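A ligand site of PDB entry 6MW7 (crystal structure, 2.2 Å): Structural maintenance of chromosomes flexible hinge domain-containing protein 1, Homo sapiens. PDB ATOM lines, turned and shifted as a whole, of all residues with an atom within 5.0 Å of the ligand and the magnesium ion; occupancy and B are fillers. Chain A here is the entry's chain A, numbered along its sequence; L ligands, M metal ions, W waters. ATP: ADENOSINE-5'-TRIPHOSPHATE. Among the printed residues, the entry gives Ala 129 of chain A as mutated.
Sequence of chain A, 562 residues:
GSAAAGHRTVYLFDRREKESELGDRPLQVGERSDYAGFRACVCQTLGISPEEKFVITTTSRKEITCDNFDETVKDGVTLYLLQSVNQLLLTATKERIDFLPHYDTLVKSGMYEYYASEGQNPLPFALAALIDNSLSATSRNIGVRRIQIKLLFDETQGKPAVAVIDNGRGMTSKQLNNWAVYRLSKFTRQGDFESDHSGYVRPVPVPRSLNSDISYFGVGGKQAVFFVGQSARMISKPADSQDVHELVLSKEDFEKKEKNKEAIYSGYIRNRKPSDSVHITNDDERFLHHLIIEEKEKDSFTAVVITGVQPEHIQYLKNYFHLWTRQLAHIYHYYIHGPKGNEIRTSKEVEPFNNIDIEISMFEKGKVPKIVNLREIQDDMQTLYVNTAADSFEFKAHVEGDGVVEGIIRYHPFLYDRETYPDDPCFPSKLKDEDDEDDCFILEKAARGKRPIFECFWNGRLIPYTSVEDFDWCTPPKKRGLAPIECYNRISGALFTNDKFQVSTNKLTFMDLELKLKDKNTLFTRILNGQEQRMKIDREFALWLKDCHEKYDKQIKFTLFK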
ATOM      1  N   ALA A 129       8.230   7.344 -10.805  1.00  0.00           N
ATOM      2  CA  ALA A 129       7.213   6.738 -11.657  1.00  0.00           C
ATOM      3  C   ALA A 129       6.590   5.510 -10.985  1.00  0.00           C
ATOM      4  O   ALA A 129       5.372   5.294 -11.074  1.00  0.00           O
ATOM      5  CB  ALA A 129       7.815   6.353 -13.010  1.00  0.00           C
ATOM      6  N   ASN A 133       2.650   4.907  -9.265  1.00  0.00           N
ATOM      7  CA  ASN A 133       1.785   3.751  -9.438  1.00  0.00           C
ATOM      8  C   ASN A 133       1.298   3.220  -8.093  1.00  0.00           C
ATOM      9  O   ASN A 133       0.111   2.882  -7.944  1.00  0.00           O
ATOM     10  CB  ASN A 133       2.515   2.655 -10.215  1.00  0.00           C
ATOM     11  CG  ASN A 133       2.755   3.026 -11.670  1.00  0.00           C
ATOM     12  OD1 ASN A 133       2.065   3.896 -12.217  1.00  0.00           O
ATOM     13  ND2 ASN A 133       3.716   2.370 -12.312  1.00  0.00           N
ATOM     14  N   SER A 134       2.177   3.150  -7.103  1.00  0.00           N
ATOM     15  CA  SER A 134       1.775   2.663  -5.783  1.00  0.00           C
ATOM     16  C   SER A 134       0.845   3.638  -5.083  1.00  0.00           C
ATOM     17  O   SER A 134      -0.059   3.219  -4.361  1.00  0.00           O
ATOM     18  CB  SER A 134       3.004   2.397  -4.921  1.00  0.00           C
ATOM     19  OG  SER A 134       3.846   1.422  -5.516  1.00  0.00           O
ATOM     20  N   ALA A 137      -2.440   2.906  -6.485  1.00  0.00           N
ATOM     21  CA  ALA A 137      -2.916   1.597  -6.073  1.00  0.00           C
ATOM     22  C   ALA A 137      -3.355   1.574  -4.619  1.00  0.00           C
ATOM     23  O   ALA A 137      -4.194   0.749  -4.247  1.00  0.00           O
ATOM     24  CB  ALA A 137      -1.839   0.548  -6.324  1.00  0.00           C
ATOM     25  N   ASP A 166       4.238  -2.339  -2.437  1.00  0.00           N
ATOM     26  CA  ASP A 166       3.171  -1.600  -1.779  1.00  0.00           C
ATOM     27  C   ASP A 166       2.093  -2.562  -1.301  1.00  0.00           C
ATOM     28  O   ASP A 166       2.051  -3.732  -1.688  1.00  0.00           O
ATOM     29  CB  ASP A 166       2.549  -0.547  -2.709  1.00  0.00           C
ATOM     30  CG  ASP A 166       1.945  -1.140  -3.955  1.00  0.00           C
ATOM     31  OD1 ASP A 166       0.817  -1.681  -3.877  1.00  0.00           O
ATOM     32  OD2 ASP A 166       2.591  -1.066  -5.019  1.00  0.00           O
ATOM     33  N   GLY A 170      -3.496  -4.258  -5.636  1.00  0.00           N
ATOM     34  CA  GLY A 170      -2.951  -5.306  -6.470  1.00  0.00           C
ATOM     35  C   GLY A 170      -3.636  -5.433  -7.824  1.00  0.00           C
ATOM     36  O   GLY A 170      -4.506  -4.645  -8.201  1.00  0.00           O
ATOM     37  N   MET A 171      -3.207  -6.457  -8.558  1.00  0.00           N
ATOM     38  CA  MET A 171      -3.683  -6.703  -9.918  1.00  0.00           C
ATOM     39  C   MET A 171      -4.166  -8.132 -10.126  1.00  0.00           C
ATOM     40  O   MET A 171      -3.477  -9.088  -9.761  1.00  0.00           O
ATOM     41  CB  MET A 171      -2.574  -6.405 -10.930  1.00  0.00           C
ATOM     42  CG  MET A 171      -2.324  -4.934 -11.196  1.00  0.00           C
ATOM     43  SD  MET A 171      -0.777  -4.679 -12.351  1.00  0.00           S
ATOM     44  CE  MET A 171       0.592  -5.159 -11.053  1.00  0.00           C
ATOM     45  N   GLN A 175      -5.588  -7.472 -15.132  1.00  0.00           N
ATOM     46  CA  GLN A 175      -4.921  -6.206 -14.868  1.00  0.00           C
ATOM     47  C   GLN A 175      -3.416  -6.329 -15.050  1.00  0.00           C
ATOM     48  O   GLN A 175      -2.772  -5.405 -15.554  1.00  0.00           O
ATOM     49  CB  GLN A 175      -5.269  -5.719 -13.460  1.00  0.00           C
ATOM     50  CG  GLN A 175      -6.751  -5.424 -13.271  1.00  0.00           C
ATOM     51  CD  GLN A 175      -7.123  -5.159 -11.838  1.00  0.00           C
ATOM     52  OE1 GLN A 175      -6.646  -5.828 -10.922  1.00  0.00           O
ATOM     53  NE2 GLN A 175      -7.989  -4.171 -11.620  1.00  0.00           N
ATOM     54  N   TRP A 179      -1.089  -4.245 -17.696  1.00  0.00           N
ATOM     55  CA  TRP A 179       0.145  -3.540 -17.365  1.00  0.00           C
ATOM     56  C   TRP A 179       1.209  -3.766 -18.428  1.00  0.00           C
ATOM     57  O   TRP A 179       1.953  -2.852 -18.783  1.00  0.00           O
ATOM     58  CB  TRP A 179       0.655  -3.999 -15.991  1.00  0.00           C
ATOM     59  CG  TRP A 179       2.078  -3.615 -15.757  1.00  0.00           C
ATOM     60  CD1 TRP A 179       2.542  -2.439 -15.244  1.00  0.00           C
ATOM     61  CD2 TRP A 179       3.246  -4.417 -16.031  1.00  0.00           C
ATOM     62  NE1 TRP A 179       3.910  -2.450 -15.184  1.00  0.00           N
ATOM     63  CE2 TRP A 179       4.365  -3.650 -15.660  1.00  0.00           C
ATOM     64  CE3 TRP A 179       3.431  -5.693 -16.559  1.00  0.00           C
ATOM     65  CZ2 TRP A 179       5.670  -4.136 -15.792  1.00  0.00           C
ATOM     66  CZ3 TRP A 179       4.728  -6.164 -16.693  1.00  0.00           C
ATOM     67  CH2 TRP A 179       5.823  -5.388 -16.301  1.00  0.00           C
ATOM     68  N   LEU A 184      -1.297   1.241 -22.974  1.00  0.00           N
ATOM     69  CA  LEU A 184      -2.639   0.952 -22.488  1.00  0.00           C
ATOM     70  C   LEU A 184      -2.838   1.701 -21.173  1.00  0.00           C
ATOM     71  O   LEU A 184      -2.199   1.387 -20.167  1.00  0.00           O
ATOM     72  CB  LEU A 184      -2.850  -0.555 -22.293  1.00  0.00           C
ATOM     73  CG  LEU A 184      -4.279  -0.940 -21.911  1.00  0.00           C
ATOM     74  CD1 LEU A 184      -5.226  -0.694 -23.083  1.00  0.00           C
ATOM     75  CD2 LEU A 184      -4.357  -2.382 -21.453  1.00  0.00           C
ATOM     76  N   SER A 185      -3.722   2.687 -21.181  1.00  0.00           N
ATOM     77  CA  SER A 185      -3.935   3.556 -20.040  1.00  0.00           C
ATOM     78  C   SER A 185      -5.336   3.352 -19.477  1.00  0.00           C
ATOM     79  O   SER A 185      -6.118   2.523 -19.961  1.00  0.00           O
ATOM     80  CB  SER A 185      -3.732   5.023 -20.438  1.00  0.00           C
ATOM     81  OG  SER A 185      -4.911   5.528 -21.036  1.00  0.00           O
ATOM     82  N   LYS A 186      -5.658   4.138 -18.453  1.00  0.00           N
ATOM     83  CA  LYS A 186      -6.979   4.112 -17.832  1.00  0.00           C
ATOM     84  C   LYS A 186      -8.063   4.601 -18.774  1.00  0.00           C
ATOM     85  O   LYS A 186      -9.247   4.360 -18.517  1.00  0.00           O
ATOM     86  CB  LYS A 186      -6.975   4.960 -16.568  1.00  0.00           C
ATOM     87  CG  LYS A 186      -6.758   6.433 -16.839  1.00  0.00           C
ATOM     88  CD  LYS A 186      -6.440   7.221 -15.579  1.00  0.00           C
ATOM     89  CE  LYS A 186      -6.444   8.709 -15.862  1.00  0.00           C
ATOM     90  NZ  LYS A 186      -5.963   9.512 -14.713  1.00  0.00           N
ATOM     91  N   ARG A 189      -8.205   0.962 -21.622  1.00  0.00           N
ATOM     92  CA  ARG A 189      -8.565  -0.399 -21.177  1.00  0.00           C
ATOM     93  C   ARG A 189     -10.031  -0.591 -20.791  1.00  0.00           C
ATOM     94  O   ARG A 189     -10.401  -1.697 -20.394  1.00  0.00           O
ATOM     95  CB  ARG A 189      -7.703  -0.824 -20.005  1.00  0.00           C
ATOM     96  CG  ARG A 189      -7.777   0.122 -18.825  1.00  0.00           C
ATOM     97  CD  ARG A 189      -7.204  -0.512 -17.610  1.00  0.00           C
ATOM     98  NE  ARG A 189      -7.211   0.368 -16.453  1.00  0.00           N
ATOM     99  CZ  ARG A 189      -6.120   0.953 -15.944  1.00  0.00           C
ATOM    100  NH1 ARG A 189      -4.923   0.779 -16.499  1.00  0.00           N
ATOM    101  NH2 ARG A 189      -6.246   1.714 -14.874  1.00  0.00           N
ATOM    102  N   ILE A 214      -2.510   9.845 -10.650  1.00  0.00           N
ATOM    103  CA  ILE A 214      -1.344  10.387 -11.339  1.00  0.00           C
ATOM    104  C   ILE A 214      -1.093   9.759 -12.702  1.00  0.00           C
ATOM    105  O   ILE A 214      -0.342  10.321 -13.506  1.00  0.00           O
ATOM    106  CB  ILE A 214      -0.113  10.217 -10.415  1.00  0.00           C
ATOM    107  CG1 ILE A 214      -0.318  11.008  -9.112  1.00  0.00           C
ATOM    108  CG2 ILE A 214       1.178  10.683 -11.097  1.00  0.00           C
ATOM    109  CD1 ILE A 214       0.701  10.715  -8.033  1.00  0.00           C
ATOM    110  N   SER A 215      -1.716   8.625 -13.008  1.00  0.00           N
ATOM    111  CA  SER A 215      -1.459   7.936 -14.267  1.00  0.00           C
ATOM    112  C   SER A 215      -2.125   8.659 -15.419  1.00  0.00           C
ATOM    113  O   SER A 215      -3.142   9.350 -15.251  1.00  0.00           O
ATOM    114  CB  SER A 215      -1.954   6.494 -14.196  1.00  0.00           C
ATOM    115  OG  SER A 215      -3.375   6.442 -14.211  1.00  0.00           O
ATOM    116  N   TYR A 216      -1.554   8.507 -16.611  1.00  0.00           N
ATOM    117  CA  TYR A 216      -2.161   9.092 -17.800  1.00  0.00           C
ATOM    118  C   TYR A 216      -1.836   8.363 -19.092  1.00  0.00           C
ATOM    119  O   TYR A 216      -2.713   8.186 -19.949  1.00  0.00           O
ATOM    120  CB  TYR A 216      -1.730  10.562 -17.937  1.00  0.00           C
ATOM    121  CG  TYR A 216      -2.780  11.415 -18.603  1.00  0.00           C
ATOM    122  CD1 TYR A 216      -3.838  11.936 -17.878  1.00  0.00           C
ATOM    123  CD2 TYR A 216      -2.726  11.676 -19.971  1.00  0.00           C
ATOM    124  CE1 TYR A 216      -4.803  12.712 -18.485  1.00  0.00           C
ATOM    125  CE2 TYR A 216      -3.691  12.451 -20.577  1.00  0.00           C
ATOM    126  CZ  TYR A 216      -4.724  12.969 -19.836  1.00  0.00           C
ATOM    127  OH  TYR A 216      -5.691  13.736 -20.447  1.00  0.00           O
ATOM    128  N   PHE A 217      -0.586   7.926 -19.269  1.00  0.00           N
ATOM    129  CA  PHE A 217      -0.116   7.507 -20.583  1.00  0.00           C
ATOM    130  C   PHE A 217      -0.041   6.004 -20.776  1.00  0.00           C
ATOM    131  O   PHE A 217      -0.009   5.538 -21.927  1.00  0.00           O
ATOM    132  CB  PHE A 217       1.262   8.099 -20.860  1.00  0.00           C
ATOM    133  CG  PHE A 217       1.343   9.576 -20.615  1.00  0.00           C
ATOM    134  CD1 PHE A 217       0.760  10.478 -21.494  1.00  0.00           C
ATOM    135  CD2 PHE A 217       2.008  10.064 -19.502  1.00  0.00           C
ATOM    136  CE1 PHE A 217       0.837  11.837 -21.264  1.00  0.00           C
ATOM    137  CE2 PHE A 217       2.085  11.423 -19.272  1.00  0.00           C
ATOM    138  CZ  PHE A 217       1.498  12.303 -20.151  1.00  0.00           C
ATOM    139  N   GLY A 218       0.006   5.219 -19.700  1.00  0.00           N
ATOM    140  CA  GLY A 218       0.154   3.786 -19.824  1.00  0.00           C
ATOM    141  C   GLY A 218       1.545   3.302 -20.186  1.00  0.00           C
ATOM    142  O   GLY A 218       1.681   2.224 -20.761  1.00  0.00           O
ATOM    143  N   VAL A 219       2.581   4.083 -19.862  1.00  0.00           N
ATOM    144  CA  VAL A 219       3.952   3.694 -20.171  1.00  0.00           C
ATOM    145  C   VAL A 219       4.912   3.887 -19.012  1.00  0.00           C
ATOM    146  O   VAL A 219       5.987   3.254 -18.999  1.00  0.00           O
ATOM    147  CB  VAL A 219       4.468   4.463 -21.408  1.00  0.00           C
ATOM    148  CG1 VAL A 219       3.491   4.360 -22.575  1.00  0.00           C
ATOM    149  CG2 VAL A 219       4.750   5.926 -21.068  1.00  0.00           C
ATOM    150  N   GLY A 220       4.600   4.720 -18.022  1.00  0.00           N
ATOM    151  CA  GLY A 220       5.614   5.184 -17.083  1.00  0.00           C
ATOM    152  C   GLY A 220       6.335   4.063 -16.365  1.00  0.00           C
ATOM    153  O   GLY A 220       7.566   4.077 -16.246  1.00  0.00           O
ATOM    154  N   GLY A 221       5.597   3.074 -15.856  1.00  0.00           N
ATOM    155  CA  GLY A 221       6.223   1.988 -15.126  1.00  0.00           C
ATOM    156  C   GLY A 221       7.186   1.189 -15.980  1.00  0.00           C
ATOM    157  O   GLY A 221       8.252   0.769 -15.512  1.00  0.00           O
ATOM    158  N   LYS A 222       6.829   0.957 -17.251  1.00  0.00           N
ATOM    159  CA  LYS A 222       7.721   0.220 -18.140  1.00  0.00           C
ATOM    160  C   LYS A 222       8.997   1.007 -18.423  1.00  0.00           C
ATOM    161  O   LYS A 222      10.091   0.443 -18.424  1.00  0.00           O
ATOM    162  CB  LYS A 222       6.998  -0.140 -19.438  1.00  0.00           C
ATOM    163  CG  LYS A 222       6.156  -1.421 -19.361  1.00  0.00           C
ATOM    164  CD  LYS A 222       4.788  -1.162 -18.755  1.00  0.00           C
ATOM    165  CE  LYS A 222       3.839  -0.563 -19.776  1.00  0.00           C
ATOM    166  NZ  LYS A 222       2.562  -0.106 -19.162  1.00  0.00           N
ATOM    167  N   MET A 234       7.030  -8.689 -12.001  1.00  0.00           N
ATOM    168  CA  MET A 234       5.838  -8.178 -11.338  1.00  0.00           C
ATOM    169  C   MET A 234       5.185  -9.273 -10.512  1.00  0.00           C
ATOM    170  O   MET A 234       4.875 -10.345 -11.031  1.00  0.00           O
ATOM    171  CB  MET A 234       4.842  -7.648 -12.376  1.00  0.00           C
ATOM    172  CG  MET A 234       5.408  -6.570 -13.278  1.00  0.00           C
ATOM    173  SD  MET A 234       5.848  -4.899 -12.364  1.00  0.00           S
ATOM    174  CE  MET A 234       4.215  -4.741 -11.299  1.00  0.00           C
ATOM    175  N   THR A 302       1.477  -5.427  -4.292  1.00  0.00           N
ATOM    176  CA  THR A 302       2.177  -5.499  -5.566  1.00  0.00           C
ATOM    177  C   THR A 302       3.660  -5.298  -5.300  1.00  0.00           C
ATOM    178  O   THR A 302       4.044  -4.428  -4.523  1.00  0.00           O
ATOM    179  CB  THR A 302       1.689  -4.458  -6.582  1.00  0.00           C
ATOM    180  OG1 THR A 302       0.318  -4.694  -6.919  1.00  0.00           O
ATOM    181  CG2 THR A 302       2.531  -4.505  -7.856  1.00  0.00           C
ATOM    182  N   LYS A 507       6.933  12.912 -17.522  1.00  0.00           N
ATOM    183  CA  LYS A 507       6.544  13.731 -16.378  1.00  0.00           C
ATOM    184  C   LYS A 507       7.740  14.486 -15.786  1.00  0.00           C
ATOM    185  O   LYS A 507       7.799  14.737 -14.581  1.00  0.00           O
ATOM    186  CB  LYS A 507       5.840  12.886 -15.320  1.00  0.00           C
ATOM    187  CG  LYS A 507       4.502  12.390 -15.832  1.00  0.00           C
ATOM    188  CD  LYS A 507       3.790  11.443 -14.895  1.00  0.00           C
ATOM    189  CE  LYS A 507       2.557  10.878 -15.598  1.00  0.00           C
ATOM    190  NZ  LYS A 507       2.061   9.627 -14.982  1.00  0.00           N
HETATM  191  PG  ATP L   1       1.698   6.542 -16.864  1.00  0.00           P
HETATM  192  O1G ATP L   1       2.418   6.342 -18.174  1.00  0.00           O
HETATM  193  O2G ATP L   1       1.187   7.944 -16.661  1.00  0.00           O
HETATM  194  O3G ATP L   1       2.471   6.009 -15.676  1.00  0.00           O
HETATM  195  PB  ATP L   1       0.209   4.223 -16.136  1.00  0.00           P
HETATM  196  O1B ATP L   1      -1.202   3.733 -16.371  1.00  0.00           O
HETATM  197  O2B ATP L   1       0.679   4.394 -14.711  1.00  0.00           O
HETATM  198  O3B ATP L   1       0.381   5.612 -16.957  1.00  0.00           O
HETATM  199  PA  ATP L   1       2.239   2.293 -16.108  1.00  0.00           P
HETATM  200  O1A ATP L   1       3.088   1.591 -17.142  1.00  0.00           O
HETATM  201  O2A ATP L   1       2.884   3.124 -15.029  1.00  0.00           O
HETATM  202  O3A ATP L   1       1.188   3.219 -16.906  1.00  0.00           O
HETATM  203  O5' ATP L   1       1.256   1.242 -15.407  1.00  0.00           O
HETATM  204  C5' ATP L   1       0.448   0.423 -16.235  1.00  0.00           C
HETATM  205  C4' ATP L   1      -0.746  -0.080 -15.440  1.00  0.00           C
HETATM  206  O4' ATP L   1      -0.364  -1.165 -14.600  1.00  0.00           O
HETATM  207  C3' ATP L   1      -1.387   0.959 -14.526  1.00  0.00           C
HETATM  208  O3' ATP L   1      -2.409   1.717 -15.179  1.00  0.00           O
HETATM  209  C2' ATP L   1      -1.956   0.120 -13.397  1.00  0.00           C
HETATM  210  O2' ATP L   1      -3.312  -0.258 -13.662  1.00  0.00           O
HETATM  211  C1' ATP L   1      -1.080  -1.114 -13.368  1.00  0.00           C
HETATM  212  N9  ATP L   1      -0.137  -0.969 -12.243  1.00  0.00           N
HETATM  213  C8  ATP L   1       1.140  -0.531 -12.321  1.00  0.00           C
HETATM  214  N7  ATP L   1       1.724  -0.526 -11.105  1.00  0.00           N
HETATM  215  C5  ATP L   1       0.805  -0.970 -10.223  1.00  0.00           C
HETATM  216  C6  ATP L   1       0.756  -1.216  -8.769  1.00  0.00           C
HETATM  217  N6  ATP L   1       1.825  -0.970  -7.988  1.00  0.00           N
HETATM  218  N1  ATP L   1      -0.395  -1.678  -8.234  1.00  0.00           N
HETATM  219  C2  ATP L   1      -1.479  -1.934  -8.983  1.00  0.00           C
HETATM  220  N3  ATP L   1      -1.502  -1.732 -10.323  1.00  0.00           N
HETATM  221  C4  ATP L   1      -0.412  -1.266 -10.971  1.00  0.00           C
HETATM  222 MG    MG M   1       2.426   5.078 -14.010  1.00  0.00          MG
HETATM  223  O   HOH W   1       4.298   5.194 -13.524  1.00  0.00           O
HETATM  224  O   HOH W   2      -1.378   3.926 -12.235  1.00  0.00           O
HETATM  225  O   HOH W   3      -0.305  -0.394 -19.125  1.00  0.00           O
HETATM  226  O   HOH W   4       4.572   8.298 -17.686  1.00  0.00           O
HETATM  227  O   HOH W   5      -3.456   5.380 -16.772  1.00  0.00           O
HETATM  228  O   HOH W   6       4.692  -0.312 -11.027  1.00  0.00           O
HETATM  229  O   HOH W   7      -3.346  -2.584 -15.374  1.00  0.00           O
HETATM  230  O   HOH W   8      -4.377  -1.936 -11.211  1.00  0.00           O
HETATM  231  O   HOH W   9      -1.142   1.741 -10.234  1.00  0.00           O
HETATM  232  O   HOH W  10       1.618   6.565 -12.845  1.00  0.00           O
HETATM  233  O   HOH W  11       4.883   0.301  -8.217  1.00  0.00           O
HETATM  234  O   HOH W  12       5.215   7.956 -14.893  1.00  0.00           O
HETATM  235  O   HOH W  13      -0.912  -2.874  -5.748  1.00  0.00           O
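The side-chain amino group (NZ) of Lys 507 lies within salt-bridge range of an oxygen (O2G) of the ligand (2.5 Å).
NZ of Lys 222 lies within salt-bridge range of O1A of the ligand, 2.7 Å away.
N of Gly 220 sits at hydrogen-bond distance from O1G of the ligand, 2.7 Å away.
The backbone NH (N) of Gly 218 is in hydrogen-bond range of an oxygen (O3B) of the ligand (2.8 Å).
The backbone NH of Tyr 216 lies within hydrogen-bond range of an oxygen (O2G) of the ligand (2.8 Å).
The backbone NH of Val 219 is in hydrogen-bond range of an oxygen (O1G) of the ligand, at 2.8 Å.
The backbone NH of Gly 221 lies within hydrogen-bond range of an oxygen (O1A) of the ligand (3.2 Å).
NH1 of Arg 189 is in hydrogen-bond range of O3' of the ligand, 3.0 Å away.
OD2 of Asp 166 sits at hydrogen-bond distance from N6 of the ligand.
The backbone NH of Phe 217 is in hydrogen-bond range of an oxygen (O2G) of the ligand (3.2 Å).
OG1 of Thr 302 sits at hydrogen-bond distance from N1 of the ligand (3.4 Å).
NZ of Lys 507 is in hydrogen-bond range of O of Ile 214 (2.9 Å).
NZ of Lys 222 is in hydrogen-bond range of O of Gly 218.
The side-chain amino group (NZ) of Lys 222 is in hydrogen-bond range of the backbone carbonyl oxygen (O) of Trp 179.
N of Asp 166 lies within hydrogen-bond range of O of Thr 302, 3.0 Å away.
OD2 of Asp 166 sits at hydrogen-bond distance from OG of Ser 134, at 2.8 Å.
The backbone carbonyl oxygen (O) of Ser 215 is in hydrogen-bond range of the side-chain amino group (NZ) of Lys 186 (2.9 Å).
A nitrogen (N3) of the ligand lies close to the side-chain sulfur of Met 171.
Merely in contact with the ligand: Ser 134 (3.99 Å), Ala 137 (3.3 Å), Trp 179 (3.2 Å) and Ser 215 (3.4 Å).
Hydrophobic or aromatic side chains that line the ligand: Ala 137, Met 171, Trp 179, Phe 217 and Val 219.
One residue has an atom within 4 Å of the magnesium ion: Asn 133.
The magnesium ion is bound by O3G of the ligand (1.9 Å), water W1 (1.9 Å), O2B of the ligand (2.0 Å), water W10 (2.1 Å), OD1 of Asn 133 (2.2 Å) and O2A of the ligand (2.3 Å).
The magnesium ion has six donor atoms within binding distance.
Water W1 lies within hydrogen-bond range of the backbone carbonyl oxygen of Ala 129, the side-chain amide nitrogen of Asn 133 and the backbone NH of Gly 221.
Water W5 lies within hydrogen-bond range of OG of Ser 215 (2.8 Å), O1B of the ligand (2.8 Å) and N of Lys 186 (3.0 Å).
Water W6 lies within hydrogen-bond range of N7 of the ligand (3.0 Å) and ND2 of Asn 133 (3.1 Å).
Water W3 lies within hydrogen-bond range of the backbone carbonyl oxygen of Leu 184 (2.8 Å), the side-chain amino group of Lys 222 (2.9 Å) and the backbone carbonyl oxygen of Trp 179 (3.4 Å).
Water W9 lies within hydrogen-bond range of O of Asn 133 (2.8 Å) and N3 of the ligand (3.5 Å).
Water W11 bridges the side-chain hydroxyl of Ser 134 (3.1 Å) and a nitrogen (N6) of the ligand (3.3 Å).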
